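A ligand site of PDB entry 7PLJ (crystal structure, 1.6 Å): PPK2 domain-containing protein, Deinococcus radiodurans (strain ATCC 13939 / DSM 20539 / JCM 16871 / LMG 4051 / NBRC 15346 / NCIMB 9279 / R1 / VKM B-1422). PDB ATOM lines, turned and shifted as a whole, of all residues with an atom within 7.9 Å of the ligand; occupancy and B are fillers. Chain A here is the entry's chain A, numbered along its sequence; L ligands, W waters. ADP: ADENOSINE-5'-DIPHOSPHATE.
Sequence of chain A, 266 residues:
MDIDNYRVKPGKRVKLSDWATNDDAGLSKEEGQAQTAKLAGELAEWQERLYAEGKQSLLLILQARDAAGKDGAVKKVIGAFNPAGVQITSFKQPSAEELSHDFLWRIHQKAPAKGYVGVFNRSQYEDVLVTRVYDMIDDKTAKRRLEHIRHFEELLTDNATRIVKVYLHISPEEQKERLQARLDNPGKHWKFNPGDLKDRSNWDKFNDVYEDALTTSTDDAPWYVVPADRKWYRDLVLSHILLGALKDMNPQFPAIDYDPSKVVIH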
ATOM      1  N   ASP A   2      14.676 -32.498 -15.179  1.00  0.00           N
ATOM      2  CA  ASP A   2      16.126 -32.541 -14.922  1.00  0.00           C
ATOM      3  C   ASP A   2      16.311 -32.510 -13.417  1.00  0.00           C
ATOM      4  O   ASP A   2      16.361 -31.425 -12.830  1.00  0.00           O
ATOM      5  CB  ASP A   2      16.835 -31.362 -15.568  1.00  0.00           C
ATOM      6  CG  ASP A   2      18.330 -31.326 -15.241  1.00  0.00           C
ATOM      7  OD1 ASP A   2      18.907 -32.338 -14.750  1.00  0.00           O
ATOM      8  OD2 ASP A   2      18.932 -30.261 -15.432  1.00  0.00           O
ATOM      9  N   ILE A   3      16.486 -33.694 -12.793  1.00  0.00           N
ATOM     10  CA  ILE A   3      16.543 -33.769 -11.334  1.00  0.00           C
ATOM     11  C   ILE A   3      17.743 -33.017 -10.790  1.00  0.00           C
ATOM     12  O   ILE A   3      17.708 -32.480  -9.669  1.00  0.00           O
ATOM     13  CB  ILE A   3      16.614 -35.250 -10.901  1.00  0.00           C
ATOM     14  CG1 ILE A   3      15.387 -35.622 -10.132  1.00  0.00           C
ATOM     15  CG2 ILE A   3      17.863 -35.572 -10.096  1.00  0.00           C
ATOM     16  CD1 ILE A   3      14.214 -35.545 -10.975  1.00  0.00           C
ATOM     17  N   ASP A   4      18.790 -32.888 -11.592  1.00  0.00           N
ATOM     18  CA  ASP A   4      19.990 -32.246 -11.102  1.00  0.00           C
ATOM     19  C   ASP A   4      19.787 -30.768 -10.854  1.00  0.00           C
ATOM     20  O   ASP A   4      20.587 -30.165 -10.141  1.00  0.00           O
ATOM     21  CB  ASP A   4      21.135 -32.455 -12.087  1.00  0.00           C
ATOM     22  CG  ASP A   4      22.488 -32.463 -11.392  1.00  0.00           C
ATOM     23  OD1 ASP A   4      22.618 -33.201 -10.389  1.00  0.00           O
ATOM     24  OD2 ASP A   4      23.398 -31.748 -11.860  1.00  0.00           O
ATOM     25  N   ASN A   5      18.763 -30.152 -11.441  1.00  0.00           N
ATOM     26  CA  ASN A   5      18.477 -28.761 -11.118  1.00  0.00           C
ATOM     27  C   ASN A   5      17.992 -28.559  -9.688  1.00  0.00           C
ATOM     28  O   ASN A   5      18.053 -27.434  -9.171  1.00  0.00           O
ATOM     29  CB  ASN A   5      17.465 -28.213 -12.130  1.00  0.00           C
ATOM     30  CG  ASN A   5      17.653 -26.750 -12.376  1.00  0.00           C
ATOM     31  OD1 ASN A   5      16.705 -25.955 -12.251  1.00  0.00           O
ATOM     32  ND2 ASN A   5      18.875 -26.363 -12.691  1.00  0.00           N
ATOM     33  N   TYR A   6      17.496 -29.608  -9.038  1.00  0.00           N
ATOM     34  CA  TYR A   6      17.118 -29.563  -7.631  1.00  0.00           C
ATOM     35  C   TYR A   6      18.283 -29.862  -6.697  1.00  0.00           C
ATOM     36  O   TYR A   6      18.130 -29.768  -5.464  1.00  0.00           O
ATOM     37  CB  TYR A   6      15.998 -30.554  -7.343  1.00  0.00           C
ATOM     38  CG  TYR A   6      14.750 -30.268  -8.158  1.00  0.00           C
ATOM     39  CD1 TYR A   6      14.282 -28.961  -8.284  1.00  0.00           C
ATOM     40  CD2 TYR A   6      14.064 -31.284  -8.798  1.00  0.00           C
ATOM     41  CE1 TYR A   6      13.113 -28.679  -9.035  1.00  0.00           C
ATOM     42  CE2 TYR A   6      12.895 -31.024  -9.559  1.00  0.00           C
ATOM     43  CZ  TYR A   6      12.423 -29.717  -9.669  1.00  0.00           C
ATOM     44  OH  TYR A   6      11.271 -29.453 -10.391  1.00  0.00           O
ATOM     45  N   ARG A   7      19.424 -30.242  -7.231  1.00  0.00           N
ATOM     46  CA  ARG A   7      20.565 -30.512  -6.375  1.00  0.00           C
ATOM     47  C   ARG A   7      21.214 -29.192  -5.947  1.00  0.00           C
ATOM     48  O   ARG A   7      21.412 -28.298  -6.767  1.00  0.00           O
ATOM     49  CB  ARG A   7      21.602 -31.407  -7.073  1.00  0.00           C
ATOM     50  CG  ARG A   7      22.843 -31.648  -6.202  1.00  0.00           C
ATOM     51  CD  ARG A   7      23.714 -32.817  -6.752  1.00  0.00           C
ATOM     52  NE  ARG A   7      24.178 -32.597  -8.123  1.00  0.00           N
ATOM     53  CZ  ARG A   7      25.324 -32.012  -8.463  1.00  0.00           C
ATOM     54  NH1 ARG A   7      26.189 -31.562  -7.558  1.00  0.00           N
ATOM     55  NH2 ARG A   7      25.622 -31.886  -9.765  1.00  0.00           N
ATOM     56  N   VAL A   8      21.534 -29.073  -4.659  1.00  0.00           N
ATOM     57  CA  VAL A   8      22.303 -27.938  -4.167  1.00  0.00           C
ATOM     58  C   VAL A   8      23.780 -28.176  -4.552  1.00  0.00           C
ATOM     59  O   VAL A   8      24.450 -29.049  -4.000  1.00  0.00           O
ATOM     60  CB  VAL A   8      22.146 -27.763  -2.653  1.00  0.00           C
ATOM     61  CG1 VAL A   8      23.042 -26.575  -2.148  1.00  0.00           C
ATOM     62  CG2 VAL A   8      20.691 -27.558  -2.256  1.00  0.00           C
ATOM     63  N   LYS A   9      24.284 -27.394  -5.502  1.00  0.00           N
ATOM     64  CA  LYS A   9      25.648 -27.608  -5.936  1.00  0.00           C
ATOM     65  C   LYS A   9      26.595 -27.125  -4.837  1.00  0.00           C
ATOM     66  O   LYS A   9      26.265 -26.195  -4.112  1.00  0.00           O
ATOM     67  CB  LYS A   9      25.902 -26.861  -7.252  1.00  0.00           C
ATOM     68  CG  LYS A   9      25.540 -27.615  -8.525  1.00  0.00           C
ATOM     69  CD  LYS A   9      24.070 -27.915  -8.676  1.00  0.00           C
ATOM     70  CE  LYS A   9      23.824 -28.649  -9.990  1.00  0.00           C
ATOM     71  NZ  LYS A   9      22.954 -27.788 -10.833  1.00  0.00           N
ATOM     72  N   PRO A  10      27.759 -27.779  -4.673  1.00  0.00           N
ATOM     73  CA  PRO A  10      28.649 -27.433  -3.545  1.00  0.00           C
ATOM     74  C   PRO A  10      29.051 -25.967  -3.537  1.00  0.00           C
ATOM     75  O   PRO A  10      29.515 -25.405  -4.557  1.00  0.00           O
ATOM     76  CB  PRO A  10      29.872 -28.341  -3.770  1.00  0.00           C
ATOM     77  CG  PRO A  10      29.388 -29.477  -4.621  1.00  0.00           C
ATOM     78  CD  PRO A  10      28.292 -28.884  -5.494  1.00  0.00           C
ATOM     79  N   GLY A  11      28.949 -25.361  -2.363  1.00  0.00           N
ATOM     80  CA  GLY A  11      29.379 -23.996  -2.203  1.00  0.00           C
ATOM     81  C   GLY A  11      28.405 -22.952  -2.717  1.00  0.00           C
ATOM     82  O   GLY A  11      28.687 -21.751  -2.605  1.00  0.00           O
ATOM     83  N   LYS A  12      27.271 -23.367  -3.297  1.00  0.00           N
ATOM     84  CA  LYS A  12      26.273 -22.432  -3.829  1.00  0.00           C
ATOM     85  C   LYS A  12      25.173 -22.330  -2.776  1.00  0.00           C
ATOM     86  O   LYS A  12      24.358 -23.249  -2.614  1.00  0.00           O
ATOM     87  CB  LYS A  12      25.711 -22.928  -5.157  1.00  0.00           C
ATOM     88  CG  LYS A  12      26.724 -23.057  -6.304  1.00  0.00           C
ATOM     89  CD  LYS A  12      27.126 -21.718  -6.852  1.00  0.00           C
ATOM     90  CE  LYS A  12      27.980 -21.889  -8.120  1.00  0.00           C
ATOM     91  NZ  LYS A  12      29.079 -22.881  -7.961  1.00  0.00           N
ATOM     92  N   ARG A  13      25.157 -21.212  -2.051  1.00  0.00           N
ATOM     93  CA  ARG A  13      24.197 -21.041  -0.971  1.00  0.00           C
ATOM     94  C   ARG A  13      22.765 -20.950  -1.510  1.00  0.00           C
ATOM     95  O   ARG A  13      22.526 -20.375  -2.582  1.00  0.00           O
ATOM     96  CB  ARG A  13      24.530 -19.798  -0.147  1.00  0.00           C
ATOM     97  CG  ARG A  13      23.668 -19.722   1.100  1.00  0.00           C
ATOM     98  CD  ARG A  13      24.026 -18.544   1.992  1.00  0.00           C
ATOM     99  NE  ARG A  13      23.039 -18.432   3.063  1.00  0.00           N
ATOM    100  CZ  ARG A  13      23.102 -19.101   4.213  1.00  0.00           C
ATOM    101  NH1 ARG A  13      24.121 -19.901   4.488  1.00  0.00           N
ATOM    102  NH2 ARG A  13      22.100 -18.988   5.079  1.00  0.00           N
ATOM    103  N   VAL A  14      21.823 -21.552  -0.781  1.00  0.00           N
ATOM    104  CA  VAL A  14      20.422 -21.564  -1.184  1.00  0.00           C
ATOM    105  C   VAL A  14      19.731 -20.356  -0.573  1.00  0.00           C
ATOM    106  O   VAL A  14      19.880 -20.071   0.616  1.00  0.00           O
ATOM    107  CB  VAL A  14      19.731 -22.867  -0.729  1.00  0.00           C
ATOM    108  CG1 VAL A  14      18.202 -22.820  -1.050  1.00  0.00           C
ATOM    109  CG2 VAL A  14      20.374 -24.101  -1.361  1.00  0.00           C
ATOM    110  N   LYS A  15      18.946 -19.650  -1.379  1.00  0.00           N
ATOM    111  CA  LYS A  15      17.939 -18.722  -0.877  1.00  0.00           C
ATOM    112  C   LYS A  15      16.594 -19.378  -1.191  1.00  0.00           C
ATOM    113  O   LYS A  15      16.150 -19.393  -2.350  1.00  0.00           O
ATOM    114  CB  LYS A  15      18.086 -17.345  -1.524  1.00  0.00           C
ATOM    115  CG  LYS A  15      17.117 -16.283  -0.978  1.00  0.00           C
ATOM    116  CD  LYS A  15      17.306 -14.995  -1.748  1.00  0.00           C
ATOM    117  CE  LYS A  15      16.407 -13.880  -1.219  1.00  0.00           C
ATOM    118  NZ  LYS A  15      16.716 -12.547  -1.859  1.00  0.00           N
ATOM    119  N   LEU A  16      15.975 -19.966  -0.174  1.00  0.00           N
ATOM    120  CA  LEU A  16      14.816 -20.838  -0.426  1.00  0.00           C
ATOM    121  C   LEU A  16      13.662 -20.104  -1.141  1.00  0.00           C
ATOM    122  O   LEU A  16      12.881 -20.735  -1.854  1.00  0.00           O
ATOM    123  CB  LEU A  16      14.331 -21.432   0.892  1.00  0.00           C
ATOM    124  CG  LEU A  16      15.178 -22.593   1.401  1.00  0.00           C
ATOM    125  CD1 LEU A  16      14.765 -22.988   2.844  1.00  0.00           C
ATOM    126  CD2 LEU A  16      15.010 -23.796   0.433  1.00  0.00           C
ATOM    127  N   SER A  17      13.520 -18.801  -0.924  1.00  0.00           N
ATOM    128  CA  SER A  17      12.440 -18.027  -1.537  1.00  0.00           C
ATOM    129  C   SER A  17      12.560 -17.929  -3.053  1.00  0.00           C
ATOM    130  O   SER A  17      11.589 -17.562  -3.723  1.00  0.00           O
ATOM    131  CB  SER A  17      12.369 -16.624  -0.949  1.00  0.00           C
ATOM    132  OG  SER A  17      13.570 -15.924  -1.218  1.00  0.00           O
ATOM    133  N   ASP A  18      13.717 -18.251  -3.609  1.00  0.00           N
ATOM    134  CA  ASP A  18      13.920 -18.277  -5.049  1.00  0.00           C
ATOM    135  C   ASP A  18      13.758 -19.675  -5.628  1.00  0.00           C
ATOM    136  O   ASP A  18      13.943 -19.858  -6.839  1.00  0.00           O
ATOM    137  CB  ASP A  18      15.323 -17.757  -5.384  1.00  0.00           C
ATOM    138  CG  ASP A  18      15.518 -16.273  -5.079  1.00  0.00           C
ATOM    139  OD1 ASP A  18      14.519 -15.518  -4.958  1.00  0.00           O
ATOM    140  OD2 ASP A  18      16.686 -15.863  -4.952  1.00  0.00           O
ATOM    141  N   TRP A  19      13.462 -20.677  -4.812  1.00  0.00           N
ATOM    142  CA  TRP A  19      13.278 -22.030  -5.309  1.00  0.00           C
ATOM    143  C   TRP A  19      11.782 -22.344  -5.311  1.00  0.00           C
ATOM    144  O   TRP A  19      11.117 -22.231  -4.278  1.00  0.00           O
ATOM    145  CB  TRP A  19      14.013 -23.033  -4.418  1.00  0.00           C
ATOM    146  CG  TRP A  19      15.520 -22.903  -4.524  1.00  0.00           C
ATOM    147  CD1 TRP A  19      16.275 -21.771  -4.277  1.00  0.00           C
ATOM    148  CD2 TRP A  19      16.440 -23.928  -4.893  1.00  0.00           C
ATOM    149  NE1 TRP A  19      17.614 -22.044  -4.489  1.00  0.00           N
ATOM    150  CE2 TRP A  19      17.736 -23.365  -4.863  1.00  0.00           C
ATOM    151  CE3 TRP A  19      16.289 -25.271  -5.271  1.00  0.00           C
ATOM    152  CZ2 TRP A  19      18.888 -24.100  -5.183  1.00  0.00           C
ATOM    153  CZ3 TRP A  19      17.429 -26.000  -5.594  1.00  0.00           C
ATOM    154  CH2 TRP A  19      18.710 -25.422  -5.539  1.00  0.00           C
ATOM    155  N   ALA A  20      11.273 -22.817  -6.446  1.00  0.00           N
ATOM    156  CA  ALA A  20       9.844 -23.069  -6.572  1.00  0.00           C
ATOM    157  C   ALA A  20       9.403 -24.195  -5.634  1.00  0.00           C
ATOM    158  O   ALA A  20      10.146 -25.137  -5.359  1.00  0.00           O
ATOM    159  CB  ALA A  20       9.469 -23.408  -7.997  1.00  0.00           C
ATOM    160  N   ASP A  23       6.476 -27.075  -8.647  1.00  0.00           N
ATOM    161  CA  ASP A  23       6.736 -27.531 -10.012  1.00  0.00           C
ATOM    162  C   ASP A  23       5.864 -28.737 -10.387  1.00  0.00           C
ATOM    163  O   ASP A  23       5.464 -29.539  -9.544  1.00  0.00           O
ATOM    164  CB  ASP A  23       8.213 -27.947 -10.182  1.00  0.00           C
ATOM    165  CG  ASP A  23       9.167 -26.756 -10.249  1.00  0.00           C
ATOM    166  OD1 ASP A  23       8.684 -25.606 -10.354  1.00  0.00           O
ATOM    167  OD2 ASP A  23      10.401 -26.971 -10.209  1.00  0.00           O
ATOM    168  N   VAL A 225      16.624 -29.963  -3.001  1.00  0.00           N
ATOM    169  CA  VAL A 225      15.494 -29.141  -2.562  1.00  0.00           C
ATOM    170  C   VAL A 225      14.329 -29.501  -3.477  1.00  0.00           C
ATOM    171  O   VAL A 225      14.263 -29.061  -4.636  1.00  0.00           O
ATOM    172  CB  VAL A 225      15.826 -27.642  -2.631  1.00  0.00           C
ATOM    173  CG1 VAL A 225      14.595 -26.764  -2.299  1.00  0.00           C
ATOM    174  CG2 VAL A 225      17.014 -27.324  -1.732  1.00  0.00           C
ATOM    175  N   PRO A 227      10.580 -29.521  -4.873  1.00  0.00           N
ATOM    176  CA  PRO A 227       9.277 -28.823  -4.832  1.00  0.00           C
ATOM    177  C   PRO A 227       8.187 -29.798  -4.437  1.00  0.00           C
ATOM    178  O   PRO A 227       7.892 -30.703  -5.246  1.00  0.00           O
ATOM    179  CB  PRO A 227       9.081 -28.347  -6.286  1.00  0.00           C
ATOM    180  CG  PRO A 227      10.402 -28.506  -6.933  1.00  0.00           C
ATOM    181  CD  PRO A 227      11.118 -29.616  -6.242  1.00  0.00           C
HETATM  182  PB  ADP L   1      24.149 -24.671 -12.894  1.00  0.00           P
HETATM  183  O1B ADP L   1      25.179 -25.581 -12.245  1.00  0.00           O
HETATM  184  O2B ADP L   1      22.895 -25.359 -13.382  1.00  0.00           O
HETATM  185  O3B ADP L   1      24.718 -23.756 -13.949  1.00  0.00           O
HETATM  186  PA  ADP L   1      24.225 -23.456 -10.273  1.00  0.00           P
HETATM  187  O1A ADP L   1      25.644 -22.948 -10.362  1.00  0.00           O
HETATM  188  O2A ADP L   1      23.922 -24.663  -9.437  1.00  0.00           O
HETATM  189  O3A ADP L   1      23.587 -23.655 -11.762  1.00  0.00           O
HETATM  190  O5' ADP L   1      23.343 -22.260  -9.620  1.00  0.00           O
HETATM  191  C5' ADP L   1      23.694 -20.874  -9.691  1.00  0.00           C
HETATM  192  C4' ADP L   1      22.674 -20.022  -8.922  1.00  0.00           C
HETATM  193  O4' ADP L   1      21.333 -20.462  -9.186  1.00  0.00           O
HETATM  194  C3' ADP L   1      22.859 -20.163  -7.421  1.00  0.00           C
HETATM  195  O3' ADP L   1      22.493 -18.908  -6.802  1.00  0.00           O
HETATM  196  C2' ADP L   1      21.846 -21.232  -7.029  1.00  0.00           C
HETATM  197  O2' ADP L   1      21.418 -21.144  -5.665  1.00  0.00           O
HETATM  198  C1' ADP L   1      20.715 -20.996  -8.000  1.00  0.00           C
HETATM  199  N9  ADP L   1      19.947 -22.240  -8.316  1.00  0.00           N
HETATM  200  C8  ADP L   1      20.444 -23.442  -8.709  1.00  0.00           C
HETATM  201  N7  ADP L   1      19.438 -24.350  -8.932  1.00  0.00           N
HETATM  202  C5  ADP L   1      18.256 -23.706  -8.667  1.00  0.00           C
HETATM  203  C6  ADP L   1      16.814 -24.040  -8.703  1.00  0.00           C
HETATM  204  N6  ADP L   1      16.341 -25.284  -9.044  1.00  0.00           N
HETATM  205  N1  ADP L   1      15.955 -23.040  -8.374  1.00  0.00           N
HETATM  206  C2  ADP L   1      16.346 -21.800  -7.998  1.00  0.00           C
HETATM  207  N3  ADP L   1      17.627 -21.429  -7.956  1.00  0.00           N
HETATM  208  C4  ADP L   1      18.611 -22.325  -8.264  1.00  0.00           C
HETATM  209  O   HOH W   1      22.421 -23.646  -4.765  1.00  0.00           O
HETATM  210  O   HOH W   2      23.736 -18.871  -4.441  1.00  0.00           O
HETATM  211  O   HOH W   3      19.552 -19.748  -4.354  1.00  0.00           O
HETATM  212  O   HOH W   4      20.858 -26.586  -8.710  1.00  0.00           O
HETATM  213  O   HOH W   5      13.148 -23.013  -9.154  1.00  0.00           O
HETATM  214  O   HOH W   6      22.819 -25.234  -6.995  1.00  0.00           O
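The side-chain amino group (NZ) of Lys 9 is in salt-bridge range of an oxygen (O1B) of the ligand, at 3.4 Å. The backbone carbonyl oxygen (O) of Arg 13 is in hydrogen-bond range of an oxygen (O2') of the ligand (3.4 Å). N6 of the ligand sits at hydrogen-bond distance from OD1 of Asn 5 (3.3 Å). O of Asn 5 lies within hydrogen-bond range of N6 of the ligand, at 2.8 Å.
Merely in contact with the ligand: Asp 18, Lys 12 and Trp 19. Hydrophobic or aromatic side chains that line the ligand: Trp 19. Of the 22 residues printed, 6 come within 4 Å of the ligand.
The backbone carbonyl oxygen (O) of Asp 4 sits at hydrogen-bond distance from the side-chain amino group (NZ) of Lys 9, 3.4 Å away.
Water W2 bridges an oxygen (O3') of the ligand and the backbone carbonyl oxygen of Arg 13. Water W3 lies within hydrogen-bond range of O2' of the ligand (2.7 Å), NE1 of Trp 19 (3.0 Å) and N of Lys 15 (3.0 Å). Water W6 lies within hydrogen-bond range of O2A of the ligand, N of Lys 9 and O of Arg 7. Water W1 bridges O2' of the ligand and O of Lys 12. Water W5 lies within hydrogen-bond range of N1 of the ligand (2.9 Å) and N of Ala 20 (3.3 Å).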
